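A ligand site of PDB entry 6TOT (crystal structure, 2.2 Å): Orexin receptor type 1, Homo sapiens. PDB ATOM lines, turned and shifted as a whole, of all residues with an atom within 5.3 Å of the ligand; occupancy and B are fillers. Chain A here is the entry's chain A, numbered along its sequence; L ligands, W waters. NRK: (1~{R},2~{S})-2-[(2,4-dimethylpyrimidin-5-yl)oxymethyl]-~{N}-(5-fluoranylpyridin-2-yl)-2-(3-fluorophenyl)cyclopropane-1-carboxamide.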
ATOM      1  N   CYS A  75      27.475 -28.541 -21.634  1.00  0.00           N
ATOM      2  CA  CYS A  75      28.354 -27.387 -21.673  1.00  0.00           C
ATOM      3  C   CYS A  75      29.589 -27.477 -20.781  1.00  0.00           C
ATOM      4  O   CYS A  75      30.621 -26.946 -21.176  1.00  0.00           O
ATOM      5  CB  CYS A  75      27.553 -26.109 -21.387  1.00  0.00           C
ATOM      6  SG  CYS A  75      25.913 -26.076 -22.181  1.00  0.00           S
ATOM      7  N   ALA A  78      32.717 -29.228 -22.575  1.00  0.00           N
ATOM      8  CA  ALA A  78      33.111 -28.312 -23.665  1.00  0.00           C
ATOM      9  C   ALA A  78      33.920 -27.116 -23.144  1.00  0.00           C
ATOM     10  O   ALA A  78      34.917 -26.767 -23.774  1.00  0.00           O
ATOM     11  CB  ALA A  78      31.872 -27.821 -24.409  1.00  0.00           C
ATOM     12  N   SER A  79      33.497 -26.520 -22.012  1.00  0.00           N
ATOM     13  CA  SER A  79      34.180 -25.405 -21.361  1.00  0.00           C
ATOM     14  C   SER A  79      35.513 -25.839 -20.827  1.00  0.00           C
ATOM     15  O   SER A  79      36.490 -25.121 -21.017  1.00  0.00           O
ATOM     16  CB  SER A  79      33.334 -24.815 -20.239  1.00  0.00           C
ATOM     17  OG  SER A  79      32.433 -23.856 -20.741  1.00  0.00           O
ATOM     18  N   VAL A  82      38.113 -26.088 -23.710  1.00  0.00           N
ATOM     19  CA  VAL A  82      38.442 -24.760 -24.255  1.00  0.00           C
ATOM     20  C   VAL A  82      39.393 -24.165 -23.180  1.00  0.00           C
ATOM     21  O   VAL A  82      40.451 -23.638 -23.519  1.00  0.00           O
ATOM     22  CB  VAL A  82      37.267 -23.797 -24.564  1.00  0.00           C
ATOM     23  CG1 VAL A  82      37.772 -22.464 -25.096  1.00  0.00           C
ATOM     24  CG2 VAL A  82      36.254 -24.424 -25.529  1.00  0.00           C
ATOM     25  N   ASP A  83      39.049 -24.323 -21.883  1.00  0.00           N
ATOM     26  CA  ASP A  83      39.869 -23.845 -20.779  1.00  0.00           C
ATOM     27  C   ASP A  83      41.258 -24.533 -20.740  1.00  0.00           C
ATOM     28  O   ASP A  83      42.204 -23.949 -20.201  1.00  0.00           O
ATOM     29  CB  ASP A  83      39.111 -23.937 -19.427  1.00  0.00           C
ATOM     30  CG  ASP A  83      38.071 -22.825 -19.135  1.00  0.00           C
ATOM     31  OD1 ASP A  83      37.951 -21.864 -19.964  1.00  0.00           O
ATOM     32  OD2 ASP A  83      37.391 -22.901 -18.074  1.00  0.00           O
ATOM     33  N   TRP A  88      38.768 -24.880 -30.252  1.00  0.00           N
ATOM     34  CA  TRP A  88      37.509 -25.603 -30.339  1.00  0.00           C
ATOM     35  C   TRP A  88      37.711 -26.921 -31.050  1.00  0.00           C
ATOM     36  O   TRP A  88      38.223 -26.936 -32.166  1.00  0.00           O
ATOM     37  CB  TRP A  88      36.436 -24.721 -30.994  1.00  0.00           C
ATOM     38  CG  TRP A  88      35.060 -25.298 -30.958  1.00  0.00           C
ATOM     39  CD1 TRP A  88      34.391 -25.853 -31.998  1.00  0.00           C
ATOM     40  CD2 TRP A  88      34.169 -25.323 -29.839  1.00  0.00           C
ATOM     41  NE1 TRP A  88      33.129 -26.237 -31.597  1.00  0.00           N
ATOM     42  CE2 TRP A  88      32.971 -25.921 -30.269  1.00  0.00           C
ATOM     43  CE3 TRP A  88      34.256 -24.841 -28.510  1.00  0.00           C
ATOM     44  CZ2 TRP A  88      31.881 -26.112 -29.421  1.00  0.00           C
ATOM     45  CZ3 TRP A  88      33.166 -25.025 -27.674  1.00  0.00           C
ATOM     46  CH2 TRP A  88      31.993 -25.648 -28.126  1.00  0.00           C
ATOM     47  N   ILE A  98      26.323 -25.496 -28.517  1.00  0.00           N
ATOM     48  CA  ILE A  98      26.751 -25.533 -27.104  1.00  0.00           C
ATOM     49  C   ILE A  98      26.761 -24.130 -26.463  1.00  0.00           C
ATOM     50  O   ILE A  98      26.096 -24.002 -25.431  1.00  0.00           O
ATOM     51  CB  ILE A  98      28.068 -26.331 -26.942  1.00  0.00           C
ATOM     52  CG1 ILE A  98      27.778 -27.820 -27.189  1.00  0.00           C
ATOM     53  CG2 ILE A  98      28.728 -26.086 -25.543  1.00  0.00           C
ATOM     54  CD1 ILE A  98      29.016 -28.739 -27.465  1.00  0.00           C
ATOM     55  N   PRO A  99      27.382 -23.043 -27.010  1.00  0.00           N
ATOM     56  CA  PRO A  99      27.282 -21.725 -26.355  1.00  0.00           C
ATOM     57  C   PRO A  99      25.824 -21.241 -26.193  1.00  0.00           C
ATOM     58  O   PRO A  99      25.506 -20.589 -25.190  1.00  0.00           O
ATOM     59  CB  PRO A  99      28.113 -20.813 -27.267  1.00  0.00           C
ATOM     60  CG  PRO A  99      29.102 -21.727 -27.896  1.00  0.00           C
ATOM     61  CD  PRO A  99      28.262 -22.946 -28.202  1.00  0.00           C
ATOM     62  N   GLN A 102      24.211 -23.172 -23.173  1.00  0.00           N
ATOM     63  CA  GLN A 102      24.749 -22.654 -21.904  1.00  0.00           C
ATOM     64  C   GLN A 102      24.130 -21.301 -21.588  1.00  0.00           C
ATOM     65  O   GLN A 102      23.740 -21.089 -20.447  1.00  0.00           O
ATOM     66  CB  GLN A 102      26.290 -22.557 -21.943  1.00  0.00           C
ATOM     67  CG  GLN A 102      26.964 -22.579 -20.557  1.00  0.00           C
ATOM     68  CD  GLN A 102      26.825 -21.311 -19.760  1.00  0.00           C
ATOM     69  OE1 GLN A 102      26.465 -21.332 -18.564  1.00  0.00           O
ATOM     70  NE2 GLN A 102      27.064 -20.171 -20.382  1.00  0.00           N
ATOM     71  N   ALA A 103      24.017 -20.406 -22.610  1.00  0.00           N
ATOM     72  CA  ALA A 103      23.343 -19.104 -22.487  1.00  0.00           C
ATOM     73  C   ALA A 103      21.852 -19.277 -22.125  1.00  0.00           C
ATOM     74  O   ALA A 103      21.351 -18.516 -21.298  1.00  0.00           O
ATOM     75  CB  ALA A 103      23.492 -18.312 -23.767  1.00  0.00           C
ATOM     76  N   VAL A 106      21.424 -20.165 -18.476  1.00  0.00           N
ATOM     77  CA  VAL A 106      21.638 -18.997 -17.599  1.00  0.00           C
ATOM     78  C   VAL A 106      20.327 -18.219 -17.511  1.00  0.00           C
ATOM     79  O   VAL A 106      19.874 -17.863 -16.419  1.00  0.00           O
ATOM     80  CB  VAL A 106      22.810 -18.094 -18.079  1.00  0.00           C
ATOM     81  CG1 VAL A 106      22.921 -16.811 -17.236  1.00  0.00           C
ATOM     82  CG2 VAL A 106      24.127 -18.857 -18.093  1.00  0.00           C
ATOM     83  N   GLN A 155      22.673 -14.872 -29.847  1.00  0.00           N
ATOM     84  CA  GLN A 155      23.921 -15.416 -29.321  1.00  0.00           C
ATOM     85  C   GLN A 155      24.413 -16.541 -30.217  1.00  0.00           C
ATOM     86  O   GLN A 155      25.597 -16.552 -30.586  1.00  0.00           O
ATOM     87  CB  GLN A 155      23.766 -15.913 -27.865  1.00  0.00           C
ATOM     88  CG  GLN A 155      25.057 -16.412 -27.214  1.00  0.00           C
ATOM     89  CD  GLN A 155      26.127 -15.334 -27.106  1.00  0.00           C
ATOM     90  OE1 GLN A 155      25.887 -14.212 -26.655  1.00  0.00           O
ATOM     91  NE2 GLN A 155      27.355 -15.645 -27.515  1.00  0.00           N
ATOM     92  N   MET A 159      28.024 -16.789 -33.188  1.00  0.00           N
ATOM     93  CA  MET A 159      29.064 -17.798 -32.956  1.00  0.00           C
ATOM     94  C   MET A 159      29.590 -18.344 -34.254  1.00  0.00           C
ATOM     95  O   MET A 159      28.805 -18.761 -35.110  1.00  0.00           O
ATOM     96  CB  MET A 159      28.574 -18.937 -32.069  1.00  0.00           C
ATOM     97  CG  MET A 159      28.091 -18.496 -30.701  1.00  0.00           C
ATOM     98  SD  MET A 159      29.252 -17.468 -29.772  1.00  0.00           S
ATOM     99  CE  MET A 159      30.633 -18.625 -29.546  1.00  0.00           C
ATOM    100  N   GLU A 180      32.604 -15.213 -31.052  1.00  0.00           N
ATOM    101  CA  GLU A 180      31.583 -14.359 -31.649  1.00  0.00           C
ATOM    102  C   GLU A 180      32.166 -13.592 -32.829  1.00  0.00           C
ATOM    103  O   GLU A 180      33.304 -13.130 -32.764  1.00  0.00           O
ATOM    104  CB  GLU A 180      31.052 -13.357 -30.619  1.00  0.00           C
ATOM    105  CG  GLU A 180      30.330 -13.955 -29.426  1.00  0.00           C
ATOM    106  CD  GLU A 180      29.896 -12.930 -28.407  1.00  0.00           C
ATOM    107  OE1 GLU A 180      30.082 -11.715 -28.645  1.00  0.00           O
ATOM    108  OE2 GLU A 180      29.343 -13.338 -27.355  1.00  0.00           O
ATOM    109  N   PHE A 195      22.881  -7.736 -22.649  1.00  0.00           N
ATOM    110  CA  PHE A 195      23.095  -9.084 -22.154  1.00  0.00           C
ATOM    111  C   PHE A 195      23.258  -9.054 -20.650  1.00  0.00           C
ATOM    112  O   PHE A 195      22.454  -9.680 -19.947  1.00  0.00           O
ATOM    113  CB  PHE A 195      24.258  -9.802 -22.862  1.00  0.00           C
ATOM    114  CG  PHE A 195      24.277 -11.288 -22.572  1.00  0.00           C
ATOM    115  CD1 PHE A 195      24.926 -11.786 -21.436  1.00  0.00           C
ATOM    116  CD2 PHE A 195      23.602 -12.184 -23.399  1.00  0.00           C
ATOM    117  CE1 PHE A 195      24.905 -13.145 -21.139  1.00  0.00           C
ATOM    118  CE2 PHE A 195      23.614 -13.555 -23.117  1.00  0.00           C
ATOM    119  CZ  PHE A 195      24.228 -14.012 -21.974  1.00  0.00           C
ATOM    120  N   TYR A 255      28.142 -15.711 -10.683  1.00  0.00           N
ATOM    121  CA  TYR A 255      27.972 -15.096 -11.996  1.00  0.00           C
ATOM    122  C   TYR A 255      28.639 -13.741 -12.129  1.00  0.00           C
ATOM    123  O   TYR A 255      28.762 -13.244 -13.252  1.00  0.00           O
ATOM    124  CB  TYR A 255      26.485 -15.032 -12.370  1.00  0.00           C
ATOM    125  CG  TYR A 255      25.954 -16.360 -12.831  1.00  0.00           C
ATOM    126  CD1 TYR A 255      25.558 -17.334 -11.912  1.00  0.00           C
ATOM    127  CD2 TYR A 255      25.899 -16.682 -14.182  1.00  0.00           C
ATOM    128  CE1 TYR A 255      25.155 -18.601 -12.328  1.00  0.00           C
ATOM    129  CE2 TYR A 255      25.477 -17.954 -14.608  1.00  0.00           C
ATOM    130  CZ  TYR A 255      25.087 -18.893 -13.678  1.00  0.00           C
ATOM    131  OH  TYR A 255      24.647 -20.133 -14.087  1.00  0.00           O
ATOM    132  N   ILE A 258      32.198 -13.736 -14.465  1.00  0.00           N
ATOM    133  CA  ILE A 258      31.960 -13.911 -15.899  1.00  0.00           C
ATOM    134  C   ILE A 258      31.253 -12.688 -16.514  1.00  0.00           C
ATOM    135  O   ILE A 258      31.652 -12.236 -17.594  1.00  0.00           O
ATOM    136  CB  ILE A 258      31.251 -15.256 -16.259  1.00  0.00           C
ATOM    137  CG1 ILE A 258      31.393 -15.572 -17.765  1.00  0.00           C
ATOM    138  CG2 ILE A 258      29.789 -15.326 -15.754  1.00  0.00           C
ATOM    139  CD1 ILE A 258      31.121 -16.986 -18.173  1.00  0.00           C
ATOM    140  N   SER A 259      30.264 -12.108 -15.793  1.00  0.00           N
ATOM    141  CA  SER A 259      29.484 -10.973 -16.257  1.00  0.00           C
ATOM    142  C   SER A 259      30.323  -9.707 -16.445  1.00  0.00           C
ATOM    143  O   SER A 259      30.225  -9.022 -17.489  1.00  0.00           O
ATOM    144  CB  SER A 259      28.308 -10.737 -15.320  1.00  0.00           C
ATOM    145  OG  SER A 259      27.505 -11.909 -15.240  1.00  0.00           O
ATOM    146  N   ASN A 262      33.111 -10.210 -19.209  1.00  0.00           N
ATOM    147  CA  ASN A 262      32.470 -10.071 -20.519  1.00  0.00           C
ATOM    148  C   ASN A 262      32.215  -8.638 -20.909  1.00  0.00           C
ATOM    149  O   ASN A 262      32.487  -8.276 -22.050  1.00  0.00           O
ATOM    150  CB  ASN A 262      31.201 -10.893 -20.646  1.00  0.00           C
ATOM    151  CG  ASN A 262      31.478 -12.151 -21.411  1.00  0.00           C
ATOM    152  OD1 ASN A 262      31.526 -12.166 -22.658  1.00  0.00           O
ATOM    153  ND2 ASN A 262      31.714 -13.243 -20.688  1.00  0.00           N
ATOM    154  N   HIS A 288      34.577 -19.170 -15.808  1.00  0.00           N
ATOM    155  CA  HIS A 288      33.764 -20.203 -16.488  1.00  0.00           C
ATOM    156  C   HIS A 288      33.454 -21.310 -15.498  1.00  0.00           C
ATOM    157  O   HIS A 288      32.303 -21.725 -15.407  1.00  0.00           O
ATOM    158  CB  HIS A 288      34.459 -20.801 -17.748  1.00  0.00           C
ATOM    159  CG  HIS A 288      34.740 -19.820 -18.843  1.00  0.00           C
ATOM    160  ND1 HIS A 288      35.923 -19.855 -19.559  1.00  0.00           N
ATOM    161  CD2 HIS A 288      34.010 -18.756 -19.265  1.00  0.00           C
ATOM    162  CE1 HIS A 288      35.859 -18.845 -20.415  1.00  0.00           C
ATOM    163  NE2 HIS A 288      34.726 -18.156 -20.286  1.00  0.00           N
ATOM    164  N   VAL A 291      30.565 -20.643 -12.854  1.00  0.00           N
ATOM    165  CA  VAL A 291      29.199 -20.726 -13.391  1.00  0.00           C
ATOM    166  C   VAL A 291      28.656 -22.148 -13.172  1.00  0.00           C
ATOM    167  O   VAL A 291      27.492 -22.325 -12.789  1.00  0.00           O
ATOM    168  CB  VAL A 291      29.189 -20.292 -14.902  1.00  0.00           C
ATOM    169  CG1 VAL A 291      27.942 -20.778 -15.628  1.00  0.00           C
ATOM    170  CG2 VAL A 291      29.341 -18.786 -15.031  1.00  0.00           C
ATOM    171  N   TYR A 292      29.524 -23.150 -13.380  1.00  0.00           N
ATOM    172  CA  TYR A 292      29.218 -24.562 -13.209  1.00  0.00           C
ATOM    173  C   TYR A 292      29.186 -24.941 -11.747  1.00  0.00           C
ATOM    174  O   TYR A 292      28.330 -25.732 -11.328  1.00  0.00           O
ATOM    175  CB  TYR A 292      30.230 -25.402 -14.014  1.00  0.00           C
ATOM    176  CG  TYR A 292      30.116 -25.132 -15.499  1.00  0.00           C
ATOM    177  CD1 TYR A 292      28.931 -25.362 -16.183  1.00  0.00           C
ATOM    178  CD2 TYR A 292      31.181 -24.565 -16.198  1.00  0.00           C
ATOM    179  CE1 TYR A 292      28.799 -25.038 -17.532  1.00  0.00           C
ATOM    180  CE2 TYR A 292      31.055 -24.234 -17.552  1.00  0.00           C
ATOM    181  CZ  TYR A 292      29.867 -24.493 -18.210  1.00  0.00           C
ATOM    182  OH  TYR A 292      29.729 -24.218 -19.547  1.00  0.00           O
HETATM  183  C01 NRK L   1      27.980 -17.240 -23.177  1.00  0.00           C
HETATM  184  C02 NRK L   1      28.608 -15.953 -23.683  1.00  0.00           C
HETATM  185  C03 NRK L   1      29.022 -16.488 -22.311  1.00  0.00           C
HETATM  186  C04 NRK L   1      30.541 -16.830 -22.186  1.00  0.00           C
HETATM  187  C05 NRK L   1      28.375 -18.718 -23.430  1.00  0.00           C
HETATM  188  C06 NRK L   1      28.486 -15.997 -20.972  1.00  0.00           C
HETATM  189  C07 NRK L   1      28.039 -16.957 -20.063  1.00  0.00           C
HETATM  190  C08 NRK L   1      27.549 -16.544 -18.833  1.00  0.00           C
HETATM  191  C09 NRK L   1      27.531 -15.212 -18.485  1.00  0.00           C
HETATM  192  C10 NRK L   1      28.022 -14.237 -19.376  1.00  0.00           C
HETATM  193  C11 NRK L   1      28.489 -14.639 -20.625  1.00  0.00           C
HETATM  194  O12 NRK L   1      30.755 -18.048 -21.445  1.00  0.00           O
HETATM  195  C13 NRK L   1      31.730 -18.972 -21.795  1.00  0.00           C
HETATM  196  C14 NRK L   1      31.741 -20.219 -21.140  1.00  0.00           C
HETATM  197  N15 NRK L   1      32.677 -21.167 -21.421  1.00  0.00           N
HETATM  198  C16 NRK L   1      33.575 -20.936 -22.421  1.00  0.00           C
HETATM  199  N17 NRK L   1      33.652 -19.787 -23.131  1.00  0.00           N
HETATM  200  C18 NRK L   1      32.726 -18.833 -22.805  1.00  0.00           C
HETATM  201  O19 NRK L   1      27.544 -19.476 -22.950  1.00  0.00           O
HETATM  202  N20 NRK L   1      29.500 -19.173 -24.028  1.00  0.00           N
HETATM  203  C21 NRK L   1      29.928 -20.526 -24.128  1.00  0.00           C
HETATM  204  C22 NRK L   1      29.503 -21.596 -23.274  1.00  0.00           C
HETATM  205  C23 NRK L   1      30.121 -22.855 -23.348  1.00  0.00           C
HETATM  206  C24 NRK L   1      31.168 -23.058 -24.268  1.00  0.00           C
HETATM  207  C25 NRK L   1      31.582 -21.972 -25.048  1.00  0.00           C
HETATM  208  N26 NRK L   1      31.004 -20.726 -24.956  1.00  0.00           N
HETATM  209  C27 NRK L   1      34.587 -22.037 -22.716  1.00  0.00           C
HETATM  210  C28 NRK L   1      30.800 -20.601 -20.006  1.00  0.00           C
HETATM  211  F29 NRK L   1      31.783 -24.267 -24.412  1.00  0.00           F
HETATM  212  F30 NRK L   1      27.129 -17.472 -17.954  1.00  0.00           F
HETATM  213  O   HOH W   1      33.876 -15.867 -21.663  1.00  0.00           O
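An oxygen (O19) of the ligand lies within hydrogen-bond range of the side-chain amide nitrogen (NE2) of Gln 102, at 2.7 Å. The side-chain hydroxyl of Ser 79 lies within hydrogen-bond range of a nitrogen (N15) of the ligand, 2.8 Å away. NE2 of His 288 sits close to N17 of the ligand (3.5 Å).
O of Pro 99 sits close to O19 of the ligand, at 3.2 Å. Merely in contact with the ligand: Val 106, Ile 258, Asn 262, Ala 78, Trp 88, Ala 103, Val 82, Ile 98, Phe 195, Tyr 255, Tyr 292 and Val 291. Hydrophobic or aromatic side chains within 4 Å of the ligand: Ala 78, Val 82, Trp 88, Ile 98, Pro 99, Val 106, Phe 195, Tyr 255, Ile 258, His 288 and Val 291.
The backbone NH of Gln 102 sits at hydrogen-bond distance from the side-chain sulfur of Cys 75. OG of Ser 79 sits at hydrogen-bond distance from OH of Tyr 292. The side-chain carboxylate (OD1) of Asp 83 lies within hydrogen-bond range of a ring nitrogen (ND1) of His 288. ND2 of Asn 262 lies within hydrogen-bond range of O of Ile 258 (3.3 Å). The side-chain hydroxyl (OG) of Ser 259 is in hydrogen-bond range of the backbone carbonyl oxygen (O) of Tyr 255. OH of Tyr 292 lies within hydrogen-bond range of O of Cys 75.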
